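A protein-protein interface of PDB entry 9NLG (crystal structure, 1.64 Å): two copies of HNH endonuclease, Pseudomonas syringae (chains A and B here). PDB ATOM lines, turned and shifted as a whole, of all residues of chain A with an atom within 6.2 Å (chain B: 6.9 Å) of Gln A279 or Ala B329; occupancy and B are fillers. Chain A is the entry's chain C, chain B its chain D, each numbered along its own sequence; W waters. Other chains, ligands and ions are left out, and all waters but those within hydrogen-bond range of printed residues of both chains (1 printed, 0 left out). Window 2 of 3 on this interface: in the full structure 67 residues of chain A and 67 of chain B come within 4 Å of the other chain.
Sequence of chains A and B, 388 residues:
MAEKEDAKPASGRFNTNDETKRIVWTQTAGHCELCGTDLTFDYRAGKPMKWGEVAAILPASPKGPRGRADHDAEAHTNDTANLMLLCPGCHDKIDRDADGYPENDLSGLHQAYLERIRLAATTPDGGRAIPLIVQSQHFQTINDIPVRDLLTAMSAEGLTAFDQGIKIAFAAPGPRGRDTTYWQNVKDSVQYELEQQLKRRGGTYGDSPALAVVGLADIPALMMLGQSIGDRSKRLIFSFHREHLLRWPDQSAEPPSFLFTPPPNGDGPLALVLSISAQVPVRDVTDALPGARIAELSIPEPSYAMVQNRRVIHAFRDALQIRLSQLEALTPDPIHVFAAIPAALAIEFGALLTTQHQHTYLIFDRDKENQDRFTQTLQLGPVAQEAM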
ATOM      1  N   VAL A 273     -20.400  -2.282  26.674  1.00  0.00           N
ATOM      2  CA  VAL A 273     -19.082  -2.590  27.211  1.00  0.00           C
ATOM      3  C   VAL A 273     -18.561  -1.335  27.895  1.00  0.00           C
ATOM      4  O   VAL A 273     -18.521  -0.262  27.283  1.00  0.00           O
ATOM      5  CB  VAL A 273     -18.119  -3.057  26.109  1.00  0.00           C
ATOM      6  CG1 VAL A 273     -16.719  -3.258  26.682  1.00  0.00           C
ATOM      7  CG2 VAL A 273     -18.636  -4.334  25.460  1.00  0.00           C
ATOM      8  N   SER A 275     -15.284   0.150  29.554  1.00  0.00           N
ATOM      9  CA  SER A 275     -13.835  -0.039  29.611  1.00  0.00           C
ATOM     10  C   SER A 275     -13.231   1.147  30.356  1.00  0.00           C
ATOM     11  O   SER A 275     -12.681   2.068  29.755  1.00  0.00           O
ATOM     12  CB  SER A 275     -13.241  -0.164  28.209  1.00  0.00           C
ATOM     13  OG  SER A 275     -13.579  -1.399  27.609  1.00  0.00           O
ATOM     14  N   ILE A 276     -13.346   1.125  31.675  1.00  0.00           N
ATOM     15  CA  ILE A 276     -12.950   2.247  32.519  1.00  0.00           C
ATOM     16  C   ILE A 276     -11.745   1.885  33.381  1.00  0.00           C
ATOM     17  O   ILE A 276     -10.739   2.595  33.384  1.00  0.00           O
ATOM     18  CB  ILE A 276     -14.139   2.728  33.385  1.00  0.00           C
ATOM     19  CG1 ILE A 276     -15.402   2.931  32.531  1.00  0.00           C
ATOM     20  CG2 ILE A 276     -13.766   3.999  34.145  1.00  0.00           C
ATOM     21  CD1 ILE A 276     -15.311   4.049  31.521  1.00  0.00           C
ATOM     22  N   SER A 277     -11.833   0.764  34.111  1.00  0.00           N
ATOM     23  CA  SER A 277     -10.693   0.243  34.861  1.00  0.00           C
ATOM     24  C   SER A 277      -9.627  -0.328  33.935  1.00  0.00           C
ATOM     25  O   SER A 277      -8.425  -0.292  34.242  1.00  0.00           O
ATOM     26  CB  SER A 277     -11.161  -0.873  35.794  1.00  0.00           C
ATOM     27  OG  SER A 277     -12.056  -0.399  36.757  1.00  0.00           O
ATOM     28  N   ALA A 278     -10.068  -0.922  32.835  1.00  0.00           N
ATOM     29  CA  ALA A 278      -9.219  -1.618  31.886  1.00  0.00           C
ATOM     30  C   ALA A 278     -10.006  -1.728  30.591  1.00  0.00           C
ATOM     31  O   ALA A 278     -11.215  -1.483  30.550  1.00  0.00           O
ATOM     32  CB  ALA A 278      -8.812  -3.000  32.400  1.00  0.00           C
ATOM     33  N   GLN A 279      -9.302  -2.113  29.534  1.00  0.00           N
ATOM     34  CA  GLN A 279      -9.917  -2.321  28.232  1.00  0.00           C
ATOM     35  C   GLN A 279     -10.535  -3.712  28.175  1.00  0.00           C
ATOM     36  O   GLN A 279      -9.817  -4.714  28.250  1.00  0.00           O
ATOM     37  CB  GLN A 279      -8.869  -2.155  27.133  1.00  0.00           C
ATOM     38  CG  GLN A 279      -9.393  -2.478  25.751  1.00  0.00           C
ATOM     39  CD  GLN A 279     -10.457  -1.513  25.313  1.00  0.00           C
ATOM     40  OE1 GLN A 279     -10.238  -0.296  25.297  1.00  0.00           O
ATOM     41  NE2 GLN A 279     -11.627  -2.037  24.965  1.00  0.00           N
ATOM     42  N   VAL A 280     -11.856  -3.783  28.032  1.00  0.00           N
ATOM     43  CA  VAL A 280     -12.508  -5.080  27.861  1.00  0.00           C
ATOM     44  C   VAL A 280     -12.241  -5.555  26.434  1.00  0.00           C
ATOM     45  O   VAL A 280     -12.584  -4.845  25.477  1.00  0.00           O
ATOM     46  CB  VAL A 280     -14.015  -5.008  28.147  1.00  0.00           C
ATOM     47  CG1 VAL A 280     -14.681  -6.355  27.836  1.00  0.00           C
ATOM     48  CG2 VAL A 280     -14.271  -4.611  29.586  1.00  0.00           C
ATOM     49  N   PRO A 281     -11.647  -6.730  26.232  1.00  0.00           N
ATOM     50  CA  PRO A 281     -11.369  -7.176  24.857  1.00  0.00           C
ATOM     51  C   PRO A 281     -12.651  -7.569  24.140  1.00  0.00           C
ATOM     52  O   PRO A 281     -13.464  -8.337  24.657  1.00  0.00           O
ATOM     53  CB  PRO A 281     -10.432  -8.378  25.047  1.00  0.00           C
ATOM     54  CG  PRO A 281      -9.912  -8.259  26.449  1.00  0.00           C
ATOM     55  CD  PRO A 281     -11.028  -7.622  27.228  1.00  0.00           C
ATOM     56  N   VAL A 282     -12.831  -7.037  22.931  1.00  0.00           N
ATOM     57  CA  VAL A 282     -14.018  -7.378  22.154  1.00  0.00           C
ATOM     58  C   VAL A 282     -14.141  -8.892  21.994  1.00  0.00           C
ATOM     59  O   VAL A 282     -15.248  -9.441  22.031  1.00  0.00           O
ATOM     60  CB  VAL A 282     -13.985  -6.662  20.791  1.00  0.00           C
ATOM     61  CG1 VAL A 282     -15.091  -7.176  19.900  1.00  0.00           C
ATOM     62  CG2 VAL A 282     -14.122  -5.156  20.995  1.00  0.00           C
ATOM     63  N   ARG A 283     -13.008  -9.589  21.837  1.00  0.00           N
ATOM     64  CA  ARG A 283     -13.049 -11.039  21.657  1.00  0.00           C
ATOM     65  C   ARG A 283     -13.767 -11.727  22.809  1.00  0.00           C
ATOM     66  O   ARG A 283     -14.440 -12.746  22.602  1.00  0.00           O
ATOM     67  CB  ARG A 283     -11.634 -11.614  21.512  1.00  0.00           C
ATOM     68  CG  ARG A 283     -10.722 -11.361  22.694  1.00  0.00           C
ATOM     69  CD  ARG A 283      -9.392 -12.086  22.576  1.00  0.00           C
ATOM     70  NE  ARG A 283      -8.651 -11.898  23.810  1.00  0.00           N
ATOM     71  CZ  ARG A 283      -7.793 -10.912  24.033  1.00  0.00           C
ATOM     72  NH1 ARG A 283      -7.344 -10.145  23.047  1.00  0.00           N
ATOM     73  NH2 ARG A 283      -7.393 -10.679  25.273  1.00  0.00           N
ATOM     74  N   GLU A 296     -19.560   0.886  23.284  1.00  0.00           N
ATOM     75  CA  GLU A 296     -18.512   0.934  24.297  1.00  0.00           C
ATOM     76  C   GLU A 296     -18.359   2.332  24.871  1.00  0.00           C
ATOM     77  O   GLU A 296     -18.218   3.305  24.126  1.00  0.00           O
ATOM     78  CB  GLU A 296     -17.161   0.472  23.739  1.00  0.00           C
ATOM     79  CG  GLU A 296     -16.049   0.511  24.786  1.00  0.00           C
ATOM     80  CD  GLU A 296     -14.742  -0.077  24.304  1.00  0.00           C
ATOM     81  OE1 GLU A 296     -14.322   0.237  23.169  1.00  0.00           O
ATOM     82  OE2 GLU A 296     -14.132  -0.858  25.064  1.00  0.00           O
ATOM     83  N   SER A 298     -15.751   4.325  27.388  1.00  0.00           N
ATOM     84  CA  SER A 298     -14.391   4.141  27.861  1.00  0.00           C
ATOM     85  C   SER A 298     -13.839   5.491  28.288  1.00  0.00           C
ATOM     86  O   SER A 298     -14.501   6.522  28.164  1.00  0.00           O
ATOM     87  CB  SER A 298     -13.513   3.508  26.779  1.00  0.00           C
ATOM     88  OG  SER A 298     -13.356   4.403  25.691  1.00  0.00           O
ATOM     89  N   PRO A 302      -7.676   3.785  30.364  1.00  0.00           N
ATOM     90  CA  PRO A 302      -8.298   2.955  31.408  1.00  0.00           C
ATOM     91  C   PRO A 302      -7.306   2.652  32.520  1.00  0.00           C
ATOM     92  O   PRO A 302      -6.145   2.345  32.269  1.00  0.00           O
ATOM     93  CB  PRO A 302      -8.721   1.693  30.648  1.00  0.00           C
ATOM     94  CG  PRO A 302      -8.960   2.192  29.244  1.00  0.00           C
ATOM     95  CD  PRO A 302      -7.906   3.236  29.014  1.00  0.00           C
ATOM     96  N   ALA A 340     -15.555  -3.556  32.998  1.00  0.00           N
ATOM     97  CA  ALA A 340     -14.335  -3.458  33.797  1.00  0.00           C
ATOM     98  C   ALA A 340     -14.356  -2.025  34.335  1.00  0.00           C
ATOM     99  O   ALA A 340     -13.892  -1.093  33.677  1.00  0.00           O
ATOM    100  CB  ALA A 340     -13.079  -3.748  32.997  1.00  0.00           C
ATOM    101  N   ARG A 366     -16.755 -11.853  34.686  1.00  0.00           N
ATOM    102  CA  ARG A 366     -15.701 -12.840  34.515  1.00  0.00           C
ATOM    103  C   ARG A 366     -15.965 -14.034  35.420  1.00  0.00           C
ATOM    104  O   ARG A 366     -16.288 -13.869  36.602  1.00  0.00           O
ATOM    105  CB  ARG A 366     -14.348 -12.223  34.846  1.00  0.00           C
ATOM    106  CG  ARG A 366     -13.954 -11.048  33.956  1.00  0.00           C
ATOM    107  CD  ARG A 366     -13.738 -11.528  32.542  1.00  0.00           C
ATOM    108  NE  ARG A 366     -13.030 -10.561  31.719  1.00  0.00           N
ATOM    109  CZ  ARG A 366     -12.542 -10.841  30.519  1.00  0.00           C
ATOM    110  NH1 ARG A 366     -12.638 -12.055  30.005  1.00  0.00           N
ATOM    111  NH2 ARG A 366     -11.954  -9.877  29.814  1.00  0.00           N
ATOM    112  N   GLN B 321      -0.340  -1.184  35.516  1.00  0.00           N
ATOM    113  CA  GLN B 321      -1.677  -1.661  35.191  1.00  0.00           C
ATOM    114  C   GLN B 321      -2.240  -0.958  33.964  1.00  0.00           C
ATOM    115  O   GLN B 321      -2.974  -1.576  33.195  1.00  0.00           O
ATOM    116  CB  GLN B 321      -2.640  -1.482  36.360  1.00  0.00           C
ATOM    117  CG  GLN B 321      -4.009  -2.103  36.111  1.00  0.00           C
ATOM    118  CD  GLN B 321      -4.987  -1.152  35.445  1.00  0.00           C
ATOM    119  OE1 GLN B 321      -4.971   0.045  35.709  1.00  0.00           O
ATOM    120  NE2 GLN B 321      -5.853  -1.689  34.597  1.00  0.00           N
ATOM    121  N   ARG B 323      -0.578  -0.217  31.392  1.00  0.00           N
ATOM    122  CA  ARG B 323      -0.008  -0.912  30.245  1.00  0.00           C
ATOM    123  C   ARG B 323      -0.477  -2.360  30.173  1.00  0.00           C
ATOM    124  O   ARG B 323      -0.725  -2.876  29.076  1.00  0.00           O
ATOM    125  CB  ARG B 323       1.513  -0.834  30.295  1.00  0.00           C
ATOM    126  CG  ARG B 323       2.029   0.596  30.328  1.00  0.00           C
ATOM    127  CD  ARG B 323       1.410   1.455  29.225  1.00  0.00           C
ATOM    128  NE  ARG B 323       1.901   2.824  29.266  1.00  0.00           N
ATOM    129  CZ  ARG B 323       1.588   3.755  28.377  1.00  0.00           C
ATOM    130  NH1 ARG B 323       0.815   3.483  27.338  1.00  0.00           N
ATOM    131  NH2 ARG B 323       2.063   4.988  28.533  1.00  0.00           N
ATOM    132  N   LEU B 324      -0.623  -3.031  31.317  1.00  0.00           N
ATOM    133  CA  LEU B 324      -1.146  -4.392  31.283  1.00  0.00           C
ATOM    134  C   LEU B 324      -2.544  -4.426  30.670  1.00  0.00           C
ATOM    135  O   LEU B 324      -2.899  -5.390  29.984  1.00  0.00           O
ATOM    136  CB  LEU B 324      -1.169  -5.002  32.683  1.00  0.00           C
ATOM    137  CG  LEU B 324       0.178  -5.286  33.335  1.00  0.00           C
ATOM    138  CD1 LEU B 324      -0.009  -6.030  34.668  1.00  0.00           C
ATOM    139  CD2 LEU B 324       1.077  -6.068  32.398  1.00  0.00           C
ATOM    140  N   SER B 325      -3.353  -3.388  30.910  1.00  0.00           N
ATOM    141  CA  SER B 325      -4.662  -3.315  30.275  1.00  0.00           C
ATOM    142  C   SER B 325      -4.524  -3.318  28.759  1.00  0.00           C
ATOM    143  O   SER B 325      -5.311  -3.957  28.057  1.00  0.00           O
ATOM    144  CB  SER B 325      -5.414  -2.070  30.742  1.00  0.00           C
ATOM    145  OG  SER B 325      -6.559  -1.815  29.936  1.00  0.00           O
ATOM    146  N   GLN B 326      -3.529  -2.602  28.240  1.00  0.00           N
ATOM    147  CA  GLN B 326      -3.310  -2.587  26.796  1.00  0.00           C
ATOM    148  C   GLN B 326      -2.810  -3.939  26.305  1.00  0.00           C
ATOM    149  O   GLN B 326      -3.286  -4.458  25.289  1.00  0.00           O
ATOM    150  CB  GLN B 326      -2.314  -1.482  26.430  1.00  0.00           C
ATOM    151  CG  GLN B 326      -2.748  -0.073  26.836  1.00  0.00           C
ATOM    152  CD  GLN B 326      -1.686   0.995  26.566  1.00  0.00           C
ATOM    153  OE1 GLN B 326      -0.493   0.711  26.498  1.00  0.00           O
ATOM    154  NE2 GLN B 326      -2.131   2.230  26.414  1.00  0.00           N
ATOM    155  N   LEU B 327      -1.832  -4.516  27.003  1.00  0.00           N
ATOM    156  CA  LEU B 327      -1.230  -5.760  26.540  1.00  0.00           C
ATOM    157  C   LEU B 327      -2.214  -6.921  26.634  1.00  0.00           C
ATOM    158  O   LEU B 327      -2.294  -7.751  25.720  1.00  0.00           O
ATOM    159  CB  LEU B 327       0.026  -6.053  27.348  1.00  0.00           C
ATOM    160  CG  LEU B 327       1.175  -5.058  27.216  1.00  0.00           C
ATOM    161  CD1 LEU B 327       2.322  -5.461  28.128  1.00  0.00           C
ATOM    162  CD2 LEU B 327       1.644  -4.964  25.766  1.00  0.00           C
ATOM    163  N   GLU B 328      -2.972  -7.003  27.730  1.00  0.00           N
ATOM    164  CA  GLU B 328      -3.941  -8.082  27.866  1.00  0.00           C
ATOM    165  C   GLU B 328      -5.004  -8.005  26.778  1.00  0.00           C
ATOM    166  O   GLU B 328      -5.488  -9.039  26.300  1.00  0.00           O
ATOM    167  CB  GLU B 328      -4.589  -8.048  29.251  1.00  0.00           C
ATOM    168  CG  GLU B 328      -3.673  -8.458  30.388  1.00  0.00           C
ATOM    169  CD  GLU B 328      -4.392  -8.497  31.732  1.00  0.00           C
ATOM    170  OE1 GLU B 328      -5.638  -8.410  31.747  1.00  0.00           O
ATOM    171  OE2 GLU B 328      -3.706  -8.588  32.770  1.00  0.00           O
ATOM    172  N   ALA B 329      -5.394  -6.788  26.382  1.00  0.00           N
ATOM    173  CA  ALA B 329      -6.366  -6.628  25.307  1.00  0.00           C
ATOM    174  C   ALA B 329      -5.778  -6.989  23.946  1.00  0.00           C
ATOM    175  O   ALA B 329      -6.524  -7.354  23.031  1.00  0.00           O
ATOM    176  CB  ALA B 329      -6.887  -5.188  25.274  1.00  0.00           C
ATOM    177  N   LEU B 330      -4.457  -6.921  23.809  1.00  0.00           N
ATOM    178  CA  LEU B 330      -3.815  -7.128  22.516  1.00  0.00           C
ATOM    179  C   LEU B 330      -3.887  -8.575  22.057  1.00  0.00           C
ATOM    180  O   LEU B 330      -3.941  -8.836  20.846  1.00  0.00           O
ATOM    181  CB  LEU B 330      -2.358  -6.677  22.620  1.00  0.00           C
ATOM    182  CG  LEU B 330      -1.557  -6.405  21.359  1.00  0.00           C
ATOM    183  CD1 LEU B 330      -2.196  -5.277  20.577  1.00  0.00           C
ATOM    184  CD2 LEU B 330      -0.138  -6.073  21.774  1.00  0.00           C
ATOM    185  N   THR B 331      -3.889  -9.527  22.991  1.00  0.00           N
ATOM    186  CA  THR B 331      -3.797 -10.932  22.640  1.00  0.00           C
ATOM    187  C   THR B 331      -4.429 -11.804  23.708  1.00  0.00           C
ATOM    188  O   THR B 331      -4.301 -11.491  24.900  1.00  0.00           O
ATOM    189  CB  THR B 331      -2.338 -11.376  22.455  1.00  0.00           C
ATOM    190  OG1 THR B 331      -2.314 -12.751  22.052  1.00  0.00           O
ATOM    191  CG2 THR B 331      -1.545 -11.229  23.753  1.00  0.00           C
ATOM    192  N   PRO B 332      -5.088 -12.903  23.321  1.00  0.00           N
ATOM    193  CA  PRO B 332      -5.555 -13.877  24.314  1.00  0.00           C
ATOM    194  C   PRO B 332      -4.438 -14.710  24.914  1.00  0.00           C
ATOM    195  O   PRO B 332      -4.675 -15.403  25.907  1.00  0.00           O
ATOM    196  CB  PRO B 332      -6.510 -14.764  23.506  1.00  0.00           C
ATOM    197  CG  PRO B 332      -5.909 -14.745  22.132  1.00  0.00           C
ATOM    198  CD  PRO B 332      -5.455 -13.314  21.949  1.00  0.00           C
ATOM    199  N   ILE B 335       1.214 -13.424  28.610  1.00  0.00           N
ATOM    200  CA  ILE B 335       2.230 -12.386  28.656  1.00  0.00           C
ATOM    201  C   ILE B 335       3.428 -12.971  29.388  1.00  0.00           C
ATOM    202  O   ILE B 335       3.300 -13.467  30.515  1.00  0.00           O
ATOM    203  CB  ILE B 335       1.700 -11.109  29.328  1.00  0.00           C
ATOM    204  CG1 ILE B 335       0.531 -10.549  28.501  1.00  0.00           C
ATOM    205  CG2 ILE B 335       2.812 -10.084  29.485  1.00  0.00           C
ATOM    206  CD1 ILE B 335      -0.218  -9.399  29.159  1.00  0.00           C
ATOM    207  N   HIS B 359      -5.720 -12.830  33.472  1.00  0.00           N
ATOM    208  CA  HIS B 359      -4.982 -13.133  32.253  1.00  0.00           C
ATOM    209  C   HIS B 359      -3.793 -14.010  32.622  1.00  0.00           C
ATOM    210  O   HIS B 359      -3.256 -13.905  33.725  1.00  0.00           O
ATOM    211  CB  HIS B 359      -4.501 -11.845  31.583  1.00  0.00           C
ATOM    212  CG  HIS B 359      -4.148 -12.003  30.138  1.00  0.00           C
ATOM    213  ND1 HIS B 359      -5.056 -11.782  29.126  1.00  0.00           N
ATOM    214  CD2 HIS B 359      -2.986 -12.343  29.533  1.00  0.00           C
ATOM    215  CE1 HIS B 359      -4.470 -11.988  27.958  1.00  0.00           C
ATOM    216  NE2 HIS B 359      -3.216 -12.339  28.177  1.00  0.00           N
HETATM  217  O   HOH W   1      -7.363  -5.400  29.043  1.00  0.00           O
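The guanidinium group (NH2) of Arg A283 is in hydrogen-bond range of the backbone carbonyl oxygen (O) of Glu B328 (2.7 Å). NH1 of Arg A283 sits at hydrogen-bond distance from O of Ala B329. NH2 of Arg A283 is in hydrogen-bond range of O of Thr B331, 3.2 Å away. The backbone NH (N) of Gln A279 lies within hydrogen-bond range of the side-chain hydroxyl (OG) of Ser B325 (2.8 Å). The side-chain amide nitrogen (NE2) of Gln B321 sits at hydrogen-bond distance from the backbone carbonyl oxygen (O) of Ser A277 (2.9 Å).
Water W1 bridges the backbone carbonyl oxygen (O) of Gln A279 (2.7 Å) and the backbone carbonyl oxygen (O) of Ser B325 (2.7 Å).
Among the printed residues, pairs that only touch across the chains: Ala A278 with Gln B321 (3.9 Å), Ala A278 with Ser B325 (3.3 Å), Gln A279 with Ala B329 (3.7 Å), Arg A283 with Leu B330 (3.9 Å) and Arg A283 with Pro B332 (3.4 Å).
The side-chain hydroxyl of Ser A275 is in hydrogen-bond range of the side-chain amide nitrogen of Gln A279. NE2 of Gln A279 is in hydrogen-bond range of OE2 of Glu A296 (2.8 Å). O of Ala A340 sits at hydrogen-bond distance from N of Ser A277, 2.8 Å away.
Of the 13 printed residues of chain B, 7 touch a printed residue of chain A. Hydrophobic or aromatic side chains of chain B within 4 Å of the printed part of chain A: Ala B329 and Pro B332. Hydrophobic or aromatic side chains of chain A that line the printed part of chain B: Ala A278. Among the printed residues, 10 pairs touch across the chains. Among the printed residues, no Asp or Glu carboxylate lies within 4 Å of a Lys or Arg side-chain nitrogen of the other chain.
Of the printed residues of chain B, Ser A277 touches Gln B321 (2.9 Å). Printed residues of chain B within 4 Å of Ala A278: Gln B321 and Ser B325. Of chain B, only Ser B325 and Ala B329 come within 4 Å of Gln A279. Printed residues of chain A within 4 Å of Glu B328: Arg A283 (2.7 Å). Printed residues of chain A within 4 Å of Ala B329: Gln A279 and Arg A283.
No position is printed for both chains.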
